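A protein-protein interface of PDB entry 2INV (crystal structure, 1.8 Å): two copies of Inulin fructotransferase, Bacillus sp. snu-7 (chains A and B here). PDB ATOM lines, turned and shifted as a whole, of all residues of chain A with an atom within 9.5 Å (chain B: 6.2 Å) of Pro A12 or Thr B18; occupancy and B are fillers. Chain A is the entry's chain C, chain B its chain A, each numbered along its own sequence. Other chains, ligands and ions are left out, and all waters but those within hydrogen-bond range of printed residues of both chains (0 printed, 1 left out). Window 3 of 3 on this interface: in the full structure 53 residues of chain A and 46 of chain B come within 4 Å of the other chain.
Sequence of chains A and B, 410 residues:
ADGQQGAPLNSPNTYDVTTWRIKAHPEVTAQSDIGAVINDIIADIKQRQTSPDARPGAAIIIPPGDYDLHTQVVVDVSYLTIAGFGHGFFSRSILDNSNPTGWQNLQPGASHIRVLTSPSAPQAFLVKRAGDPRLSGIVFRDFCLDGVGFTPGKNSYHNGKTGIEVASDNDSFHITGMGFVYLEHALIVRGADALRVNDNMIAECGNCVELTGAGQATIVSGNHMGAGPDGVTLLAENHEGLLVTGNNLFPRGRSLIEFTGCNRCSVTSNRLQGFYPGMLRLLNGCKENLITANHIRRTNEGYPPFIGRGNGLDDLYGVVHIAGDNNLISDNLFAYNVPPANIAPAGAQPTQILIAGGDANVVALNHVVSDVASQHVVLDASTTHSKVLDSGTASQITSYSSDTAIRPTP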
ATOM      1  N   PRO A  12      10.240  13.912  11.351  1.00  0.00           N
ATOM      2  CA  PRO A  12      10.607  12.889  10.350  1.00  0.00           C
ATOM      3  C   PRO A  12      11.344  11.669  10.904  1.00  0.00           C
ATOM      4  O   PRO A  12      12.289  11.792  11.687  1.00  0.00           O
ATOM      5  CB  PRO A  12      11.425  13.618   9.309  1.00  0.00           C
ATOM      6  CG  PRO A  12      10.680  14.960   9.274  1.00  0.00           C
ATOM      7  CD  PRO A  12      10.236  15.249  10.726  1.00  0.00           C
ATOM      8  N   ASN A  13      10.880  10.496  10.485  1.00  0.00           N
ATOM      9  CA  ASN A  13      11.448   9.223  10.908  1.00  0.00           C
ATOM     10  C   ASN A  13      11.457   9.087  12.423  1.00  0.00           C
ATOM     11  O   ASN A  13      12.278   8.356  12.992  1.00  0.00           O
ATOM     12  CB  ASN A  13      12.869   9.066  10.371  1.00  0.00           C
ATOM     13  CG  ASN A  13      12.899   8.797   8.869  1.00  0.00           C
ATOM     14  OD1 ASN A  13      13.778   9.282   8.165  1.00  0.00           O
ATOM     15  ND2 ASN A  13      11.939   8.021   8.379  1.00  0.00           N
ATOM     16  N   THR A  14      10.539   9.790  13.077  1.00  0.00           N
ATOM     17  CA  THR A  14      10.430   9.732  14.534  1.00  0.00           C
ATOM     18  C   THR A  14       8.995   9.342  14.874  1.00  0.00           C
ATOM     19  O   THR A  14       8.044   9.957  14.369  1.00  0.00           O
ATOM     20  CB  THR A  14      10.720  11.105  15.190  1.00  0.00           C
ATOM     21  OG1 THR A  14      11.964  11.625  14.707  1.00  0.00           O
ATOM     22  CG2 THR A  14      10.800  10.965  16.701  1.00  0.00           C
ATOM     23  N   TYR A  15       8.838   8.305  15.696  1.00  0.00           N
ATOM     24  CA  TYR A  15       7.508   7.869  16.106  1.00  0.00           C
ATOM     25  C   TYR A  15       7.446   7.891  17.635  1.00  0.00           C
ATOM     26  O   TYR A  15       8.470   7.781  18.313  1.00  0.00           O
ATOM     27  CB  TYR A  15       7.205   6.432  15.657  1.00  0.00           C
ATOM     28  CG  TYR A  15       7.411   6.100  14.189  1.00  0.00           C
ATOM     29  CD1 TYR A  15       8.692   5.989  13.644  1.00  0.00           C
ATOM     30  CD2 TYR A  15       6.322   5.819  13.364  1.00  0.00           C
ATOM     31  CE1 TYR A  15       8.884   5.603  12.324  1.00  0.00           C
ATOM     32  CE2 TYR A  15       6.506   5.424  12.035  1.00  0.00           C
ATOM     33  CZ  TYR A  15       7.785   5.319  11.522  1.00  0.00           C
ATOM     34  OH  TYR A  15       7.982   4.929  10.214  1.00  0.00           O
ATOM     35  N   ASP A  44       6.145   0.292   8.733  1.00  0.00           N
ATOM     36  CA  ASP A  44       5.980   1.565   8.037  1.00  0.00           C
ATOM     37  C   ASP A  44       7.328   2.122   7.603  1.00  0.00           C
ATOM     38  O   ASP A  44       7.423   2.803   6.580  1.00  0.00           O
ATOM     39  CB  ASP A  44       5.293   2.600   8.920  1.00  0.00           C
ATOM     40  CG  ASP A  44       5.031   3.912   8.176  1.00  0.00           C
ATOM     41  OD1 ASP A  44       4.120   3.953   7.316  1.00  0.00           O
ATOM     42  OD2 ASP A  44       5.752   4.898   8.446  1.00  0.00           O
ATOM     43  N   ILE A  45       8.367   1.823   8.379  1.00  0.00           N
ATOM     44  CA  ILE A  45       9.711   2.289   8.066  1.00  0.00           C
ATOM     45  C   ILE A  45      10.164   1.597   6.788  1.00  0.00           C
ATOM     46  O   ILE A  45      10.664   2.242   5.866  1.00  0.00           O
ATOM     47  CB  ILE A  45      10.696   1.950   9.202  1.00  0.00           C
ATOM     48  CG1 ILE A  45      10.324   2.739  10.457  1.00  0.00           C
ATOM     49  CG2 ILE A  45      12.126   2.260   8.774  1.00  0.00           C
ATOM     50  CD1 ILE A  45      11.164   2.392  11.677  1.00  0.00           C
ATOM     51  N   ARG A  48       8.370   2.854   3.741  1.00  0.00           N
ATOM     52  CA  ARG A  48       8.973   4.065   3.241  1.00  0.00           C
ATOM     53  C   ARG A  48      10.413   4.004   2.735  1.00  0.00           C
ATOM     54  O   ARG A  48      10.715   4.570   1.684  1.00  0.00           O
ATOM     55  CB  ARG A  48       8.812   5.136   4.319  1.00  0.00           C
ATOM     56  CG  ARG A  48       7.341   5.424   4.605  1.00  0.00           C
ATOM     57  CD  ARG A  48       7.097   6.513   5.651  1.00  0.00           C
ATOM     58  NE  ARG A  48       7.826   6.262   6.888  1.00  0.00           N
ATOM     59  CZ  ARG A  48       9.050   6.718   7.131  1.00  0.00           C
ATOM     60  NH1 ARG A  48       9.677   7.453   6.220  1.00  0.00           N
ATOM     61  NH2 ARG A  48       9.647   6.440   8.282  1.00  0.00           N
ATOM     62  N   GLN A  49      11.302   3.324   3.450  1.00  0.00           N
ATOM     63  CA  GLN A  49      12.689   3.249   3.009  1.00  0.00           C
ATOM     64  C   GLN A  49      12.971   1.938   2.278  1.00  0.00           C
ATOM     65  O   GLN A  49      13.402   0.948   2.872  1.00  0.00           O
ATOM     66  CB  GLN A  49      13.614   3.436   4.214  1.00  0.00           C
ATOM     67  CG  GLN A  49      13.185   4.620   5.068  1.00  0.00           C
ATOM     68  CD  GLN A  49      14.028   4.842   6.305  1.00  0.00           C
ATOM     69  OE1 GLN A  49      13.758   5.757   7.091  1.00  0.00           O
ATOM     70  NE2 GLN A  49      15.071   4.031   6.476  1.00  0.00           N
ATOM     71  N   PRO A  56      18.142   5.316   6.262  1.00  0.00           N
ATOM     72  CA  PRO A  56      18.587   6.105   7.416  1.00  0.00           C
ATOM     73  C   PRO A  56      18.171   5.455   8.721  1.00  0.00           C
ATOM     74  O   PRO A  56      18.891   5.514   9.724  1.00  0.00           O
ATOM     75  CB  PRO A  56      17.861   7.429   7.215  1.00  0.00           C
ATOM     76  CG  PRO A  56      17.913   7.590   5.755  1.00  0.00           C
ATOM     77  CD  PRO A  56      17.578   6.208   5.229  1.00  0.00           C
ATOM     78  N   GLY A  57      16.987   4.851   8.697  1.00  0.00           N
ATOM     79  CA  GLY A  57      16.469   4.204   9.883  1.00  0.00           C
ATOM     80  C   GLY A  57      15.460   5.138  10.507  1.00  0.00           C
ATOM     81  O   GLY A  57      14.882   5.985   9.824  1.00  0.00           O
ATOM     82  N   ALA A  58      15.241   4.990  11.805  1.00  0.00           N
ATOM     83  CA  ALA A  58      14.295   5.840  12.484  1.00  0.00           C
ATOM     84  C   ALA A  58      14.465   5.750  13.980  1.00  0.00           C
ATOM     85  O   ALA A  58      15.308   5.013  14.488  1.00  0.00           O
ATOM     86  CB  ALA A  58      12.877   5.449  12.091  1.00  0.00           C
ATOM     87  N   ALA A  59      13.651   6.524  14.679  1.00  0.00           N
ATOM     88  CA  ALA A  59      13.674   6.540  16.121  1.00  0.00           C
ATOM     89  C   ALA A  59      12.266   6.317  16.644  1.00  0.00           C
ATOM     90  O   ALA A  59      11.319   6.988  16.225  1.00  0.00           O
ATOM     91  CB  ALA A  59      14.210   7.871  16.614  1.00  0.00           C
ATOM     92  N   ILE A  60      12.139   5.346  17.539  1.00  0.00           N
ATOM     93  CA  ILE A  60      10.871   5.028  18.167  1.00  0.00           C
ATOM     94  C   ILE A  60      11.022   5.417  19.635  1.00  0.00           C
ATOM     95  O   ILE A  60      11.881   4.888  20.346  1.00  0.00           O
ATOM     96  CB  ILE A  60      10.553   3.524  18.043  1.00  0.00           C
ATOM     97  CG1 ILE A  60      10.485   3.128  16.564  1.00  0.00           C
ATOM     98  CG2 ILE A  60       9.235   3.206  18.732  1.00  0.00           C
ATOM     99  CD1 ILE A  60      10.210   1.660  16.319  1.00  0.00           C
ATOM    100  N   ILE A  61      10.204   6.375  20.056  1.00  0.00           N
ATOM    101  CA  ILE A  61      10.216   6.898  21.415  1.00  0.00           C
ATOM    102  C   ILE A  61       9.165   6.222  22.292  1.00  0.00           C
ATOM    103  O   ILE A  61       8.018   6.061  21.864  1.00  0.00           O
ATOM    104  CB  ILE A  61       9.917   8.412  21.405  1.00  0.00           C
ATOM    105  CG1 ILE A  61      10.879   9.134  20.464  1.00  0.00           C
ATOM    106  CG2 ILE A  61       9.979   8.964  22.818  1.00  0.00           C
ATOM    107  CD1 ILE A  61      12.344   8.888  20.758  1.00  0.00           C
ATOM    108  N   ASP B  16      14.332  21.927  15.085  1.00  0.00           N
ATOM    109  CA  ASP B  16      14.384  20.599  14.468  1.00  0.00           C
ATOM    110  C   ASP B  16      14.891  20.994  13.079  1.00  0.00           C
ATOM    111  O   ASP B  16      14.258  21.808  12.412  1.00  0.00           O
ATOM    112  CB  ASP B  16      12.977  20.019  14.339  1.00  0.00           C
ATOM    113  CG  ASP B  16      12.942  18.734  13.525  1.00  0.00           C
ATOM    114  OD1 ASP B  16      13.483  18.728  12.398  1.00  0.00           O
ATOM    115  OD2 ASP B  16      12.352  17.731  13.993  1.00  0.00           O
ATOM    116  N   VAL B  17      16.022  20.465  12.628  1.00  0.00           N
ATOM    117  CA  VAL B  17      16.505  20.899  11.323  1.00  0.00           C
ATOM    118  C   VAL B  17      15.523  20.716  10.166  1.00  0.00           C
ATOM    119  O   VAL B  17      15.560  21.500   9.215  1.00  0.00           O
ATOM    120  CB  VAL B  17      17.873  20.252  10.933  1.00  0.00           C
ATOM    121  CG1 VAL B  17      18.971  20.765  11.845  1.00  0.00           C
ATOM    122  CG2 VAL B  17      17.790  18.742  10.972  1.00  0.00           C
ATOM    123  N   THR B  18      14.622  19.739  10.248  1.00  0.00           N
ATOM    124  CA  THR B  18      13.682  19.518   9.146  1.00  0.00           C
ATOM    125  C   THR B  18      12.481  20.477   9.025  1.00  0.00           C
ATOM    126  O   THR B  18      11.898  20.579   7.945  1.00  0.00           O
ATOM    127  CB  THR B  18      13.121  18.068   9.164  1.00  0.00           C
ATOM    128  OG1 THR B  18      12.214  17.911  10.263  1.00  0.00           O
ATOM    129  CG2 THR B  18      14.255  17.059   9.309  1.00  0.00           C
ATOM    130  N   THR B  19      12.112  21.180  10.097  1.00  0.00           N
ATOM    131  CA  THR B  19      10.958  22.089  10.045  1.00  0.00           C
ATOM    132  C   THR B  19      11.313  23.548   9.815  1.00  0.00           C
ATOM    133  O   THR B  19      10.447  24.369   9.516  1.00  0.00           O
ATOM    134  CB  THR B  19      10.173  22.093  11.364  1.00  0.00           C
ATOM    135  OG1 THR B  19      11.058  22.433  12.441  1.00  0.00           O
ATOM    136  CG2 THR B  19       9.540  20.748  11.627  1.00  0.00           C
ATOM    137  N   TRP B  20      12.588  23.869   9.964  1.00  0.00           N
ATOM    138  CA  TRP B  20      13.031  25.239   9.852  1.00  0.00           C
ATOM    139  C   TRP B  20      13.376  25.750   8.455  1.00  0.00           C
ATOM    140  O   TRP B  20      14.369  25.331   7.853  1.00  0.00           O
ATOM    141  CB  TRP B  20      14.200  25.415  10.817  1.00  0.00           C
ATOM    142  CG  TRP B  20      14.829  26.727  10.731  1.00  0.00           C
ATOM    143  CD1 TRP B  20      15.796  27.109   9.859  1.00  0.00           C
ATOM    144  CD2 TRP B  20      14.531  27.865  11.534  1.00  0.00           C
ATOM    145  NE1 TRP B  20      16.124  28.421  10.063  1.00  0.00           N
ATOM    146  CE2 TRP B  20      15.359  28.913  11.086  1.00  0.00           C
ATOM    147  CE3 TRP B  20      13.633  28.104  12.584  1.00  0.00           C
ATOM    148  CZ2 TRP B  20      15.332  30.185  11.659  1.00  0.00           C
ATOM    149  CZ3 TRP B  20      13.601  29.371  13.156  1.00  0.00           C
ATOM    150  CH2 TRP B  20      14.447  30.397  12.688  1.00  0.00           C
ATOM    151  N   ARG B  21      12.564  26.681   7.957  1.00  0.00           N
ATOM    152  CA  ARG B  21      12.783  27.235   6.624  1.00  0.00           C
ATOM    153  C   ARG B  21      13.688  28.457   6.644  1.00  0.00           C
ATOM    154  O   ARG B  21      13.643  29.273   7.578  1.00  0.00           O
ATOM    155  CB  ARG B  21      11.448  27.611   5.974  1.00  0.00           C
ATOM    156  CG  ARG B  21      10.680  28.742   6.649  1.00  0.00           C
ATOM    157  CD  ARG B  21       9.448  29.141   5.846  1.00  0.00           C
ATOM    158  NE  ARG B  21       8.682  30.192   6.510  1.00  0.00           N
ATOM    159  CZ  ARG B  21       7.543  30.693   6.039  1.00  0.00           C
ATOM    160  NH1 ARG B  21       7.028  30.238   4.897  1.00  0.00           N
ATOM    161  NH2 ARG B  21       6.909  31.650   6.709  1.00  0.00           N
ATOM    162  N   ALA B  30      17.354  20.767   4.923  1.00  0.00           N
ATOM    163  CA  ALA B  30      18.396  20.031   5.621  1.00  0.00           C
ATOM    164  C   ALA B  30      18.917  18.944   4.686  1.00  0.00           C
ATOM    165  O   ALA B  30      20.093  18.591   4.732  1.00  0.00           O
ATOM    166  CB  ALA B  30      17.846  19.408   6.899  1.00  0.00           C
ATOM    167  N   VAL B  37      21.147  25.398   6.625  1.00  0.00           N
ATOM    168  CA  VAL B  37      20.057  25.403   7.590  1.00  0.00           C
ATOM    169  C   VAL B  37      20.528  25.728   8.995  1.00  0.00           C
ATOM    170  O   VAL B  37      19.965  26.599   9.660  1.00  0.00           O
ATOM    171  CB  VAL B  37      19.345  24.034   7.616  1.00  0.00           C
ATOM    172  CG1 VAL B  37      18.204  24.050   8.609  1.00  0.00           C
ATOM    173  CG2 VAL B  37      18.840  23.694   6.222  1.00  0.00           C
ATOM    174  N   ILE B  61      18.039  19.870  16.984  1.00  0.00           N
ATOM    175  CA  ILE B  61      17.774  18.439  16.862  1.00  0.00           C
ATOM    176  C   ILE B  61      17.868  17.965  15.416  1.00  0.00           C
ATOM    177  O   ILE B  61      17.311  18.609  14.516  1.00  0.00           O
ATOM    178  CB  ILE B  61      16.354  18.110  17.370  1.00  0.00           C
ATOM    179  CG1 ILE B  61      16.187  18.599  18.808  1.00  0.00           C
ATOM    180  CG2 ILE B  61      16.083  16.625  17.246  1.00  0.00           C
ATOM    181  CD1 ILE B  61      17.218  18.068  19.776  1.00  0.00           C
ATOM    182  N   ILE B  62      18.554  16.846  15.182  1.00  0.00           N
ATOM    183  CA  ILE B  62      18.660  16.335  13.821  1.00  0.00           C
ATOM    184  C   ILE B  62      17.973  14.973  13.709  1.00  0.00           C
ATOM    185  O   ILE B  62      18.530  13.943  14.095  1.00  0.00           O
ATOM    186  CB  ILE B  62      20.129  16.208  13.376  1.00  0.00           C
ATOM    187  CG1 ILE B  62      20.814  17.576  13.471  1.00  0.00           C
ATOM    188  CG2 ILE B  62      20.201  15.711  11.930  1.00  0.00           C
ATOM    189  CD1 ILE B  62      22.330  17.532  13.376  1.00  0.00           C
ATOM    190  N   PRO B  63      16.728  14.963  13.209  1.00  0.00           N
ATOM    191  CA  PRO B  63      15.889  13.774  13.007  1.00  0.00           C
ATOM    192  C   PRO B  63      16.558  12.655  12.197  1.00  0.00           C
ATOM    193  O   PRO B  63      17.496  12.896  11.441  1.00  0.00           O
ATOM    194  CB  PRO B  63      14.680  14.340  12.275  1.00  0.00           C
ATOM    195  CG  PRO B  63      14.493  15.643  12.962  1.00  0.00           C
ATOM    196  CD  PRO B  63      15.915  16.192  13.096  1.00  0.00           C
ATOM    197  N   PRO B  64      16.108  11.405  12.387  1.00  0.00           N
ATOM    198  CA  PRO B  64      16.701  10.305  11.625  1.00  0.00           C
ATOM    199  C   PRO B  64      16.623  10.646  10.142  1.00  0.00           C
ATOM    200  O   PRO B  64      15.555  10.963   9.641  1.00  0.00           O
ATOM    201  CB  PRO B  64      15.807   9.118  11.990  1.00  0.00           C
ATOM    202  CG  PRO B  64      15.528   9.387  13.428  1.00  0.00           C
ATOM    203  CD  PRO B  64      15.280  10.890  13.493  1.00  0.00           C
ATOM    204  N   GLY B  65      17.745  10.573   9.438  1.00  0.00           N
ATOM    205  CA  GLY B  65      17.706  10.879   8.023  1.00  0.00           C
ATOM    206  C   GLY B  65      19.017  11.103   7.312  1.00  0.00           C
ATOM    207  O   GLY B  65      20.082  11.154   7.916  1.00  0.00           O
ATOM    208  N   TYR B  67      21.171  13.622   5.235  1.00  0.00           N
ATOM    209  CA  TYR B  67      21.329  15.057   4.994  1.00  0.00           C
ATOM    210  C   TYR B  67      22.691  15.402   4.388  1.00  0.00           C
ATOM    211  O   TYR B  67      23.729  14.968   4.889  1.00  0.00           O
ATOM    212  CB  TYR B  67      21.179  15.835   6.306  1.00  0.00           C
ATOM    213  CG  TYR B  67      19.975  15.450   7.126  1.00  0.00           C
ATOM    214  CD1 TYR B  67      18.710  15.944   6.821  1.00  0.00           C
ATOM    215  CD2 TYR B  67      20.101  14.583   8.208  1.00  0.00           C
ATOM    216  CE1 TYR B  67      17.595  15.582   7.576  1.00  0.00           C
ATOM    217  CE2 TYR B  67      18.998  14.216   8.971  1.00  0.00           C
ATOM    218  CZ  TYR B  67      17.749  14.718   8.650  1.00  0.00           C
ATOM    219  OH  TYR B  67      16.661  14.353   9.399  1.00  0.00           O
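The backbone carbonyl oxygen (O) of Pro B63 is in hydrogen-bond range of the side-chain hydroxyl (OH) of Tyr B67 (2.6 Å). The side-chain hydroxyl of Thr A14 is in hydrogen-bond range of the backbone carbonyl oxygen of Pro A12 (3.0 Å). NH2 of Arg A48 sits close to ND2 of Asn A13, at 2.8 Å. O of Asn A13 is in hydrogen-bond range of N of Ala A59, at 2.8 Å. The backbone NH (N) of Tyr A15 sits at hydrogen-bond distance from the backbone carbonyl oxygen (O) of Ala A59 (2.9 Å). OE1 of Gln A49 lies close to O of Gly A57 (3.0 Å).
Of chain A, only Pro A12 comes within 4 Å of Thr B18. No residue of chain A comes within 4 Å of Asp B16. Val B17 touches none of the printed residues of chain A. No residue of chain A comes within 4 Å of Thr B19. Pro B64 touches just these residues of chain A: Pro A12 (3.6 Å), Asn A13 (2.9 Å), Thr A14 (3.6 Å), Gly A57 (3.9 Å), Ala A58 (3.6 Å) and Ala A59 (3.6 Å). Of the printed residues of chain B, Gly A57 touches Pro B64. Of the printed residues of chain B, Pro A56 touches Gly B65. The nearest residue of chain B that does not touch Pro A12 is Asp B16 (4.6 Å). The nearest residue of chain A that does not touch Thr B18 is Asn A13 (7.5 Å).
Pro A12 touches Thr B18 (CD to OG1, 3.3 Å). Pro B63 touches Pro A12 (CB to O, 3.5 Å). Pro A12 touches Pro B64. Pro B64 touches Thr A14 (CD to OG1, 3.6 Å). Gly B65 touches Pro A56 (CA to CB, 3.5 Å). Pro B64 touches Gly A57. Pro B64 touches Ala A58 (CB to CA, 3.6 Å). N of Ala A59 touches CG of Pro B64, 3.6 Å away.
Of the 14 printed residues of chain A, 7 touch a printed residue of chain B. Among the printed residues, 9 pairs touch across the chains. Among the printed residues, no Asp or Glu carboxylate lies within 4 Å of a Lys or Arg side-chain nitrogen of the other chain.
Position printed for both chains: 61.
O of Pro B64 lies close to OD1 of Asn A13 (2.9 Å).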
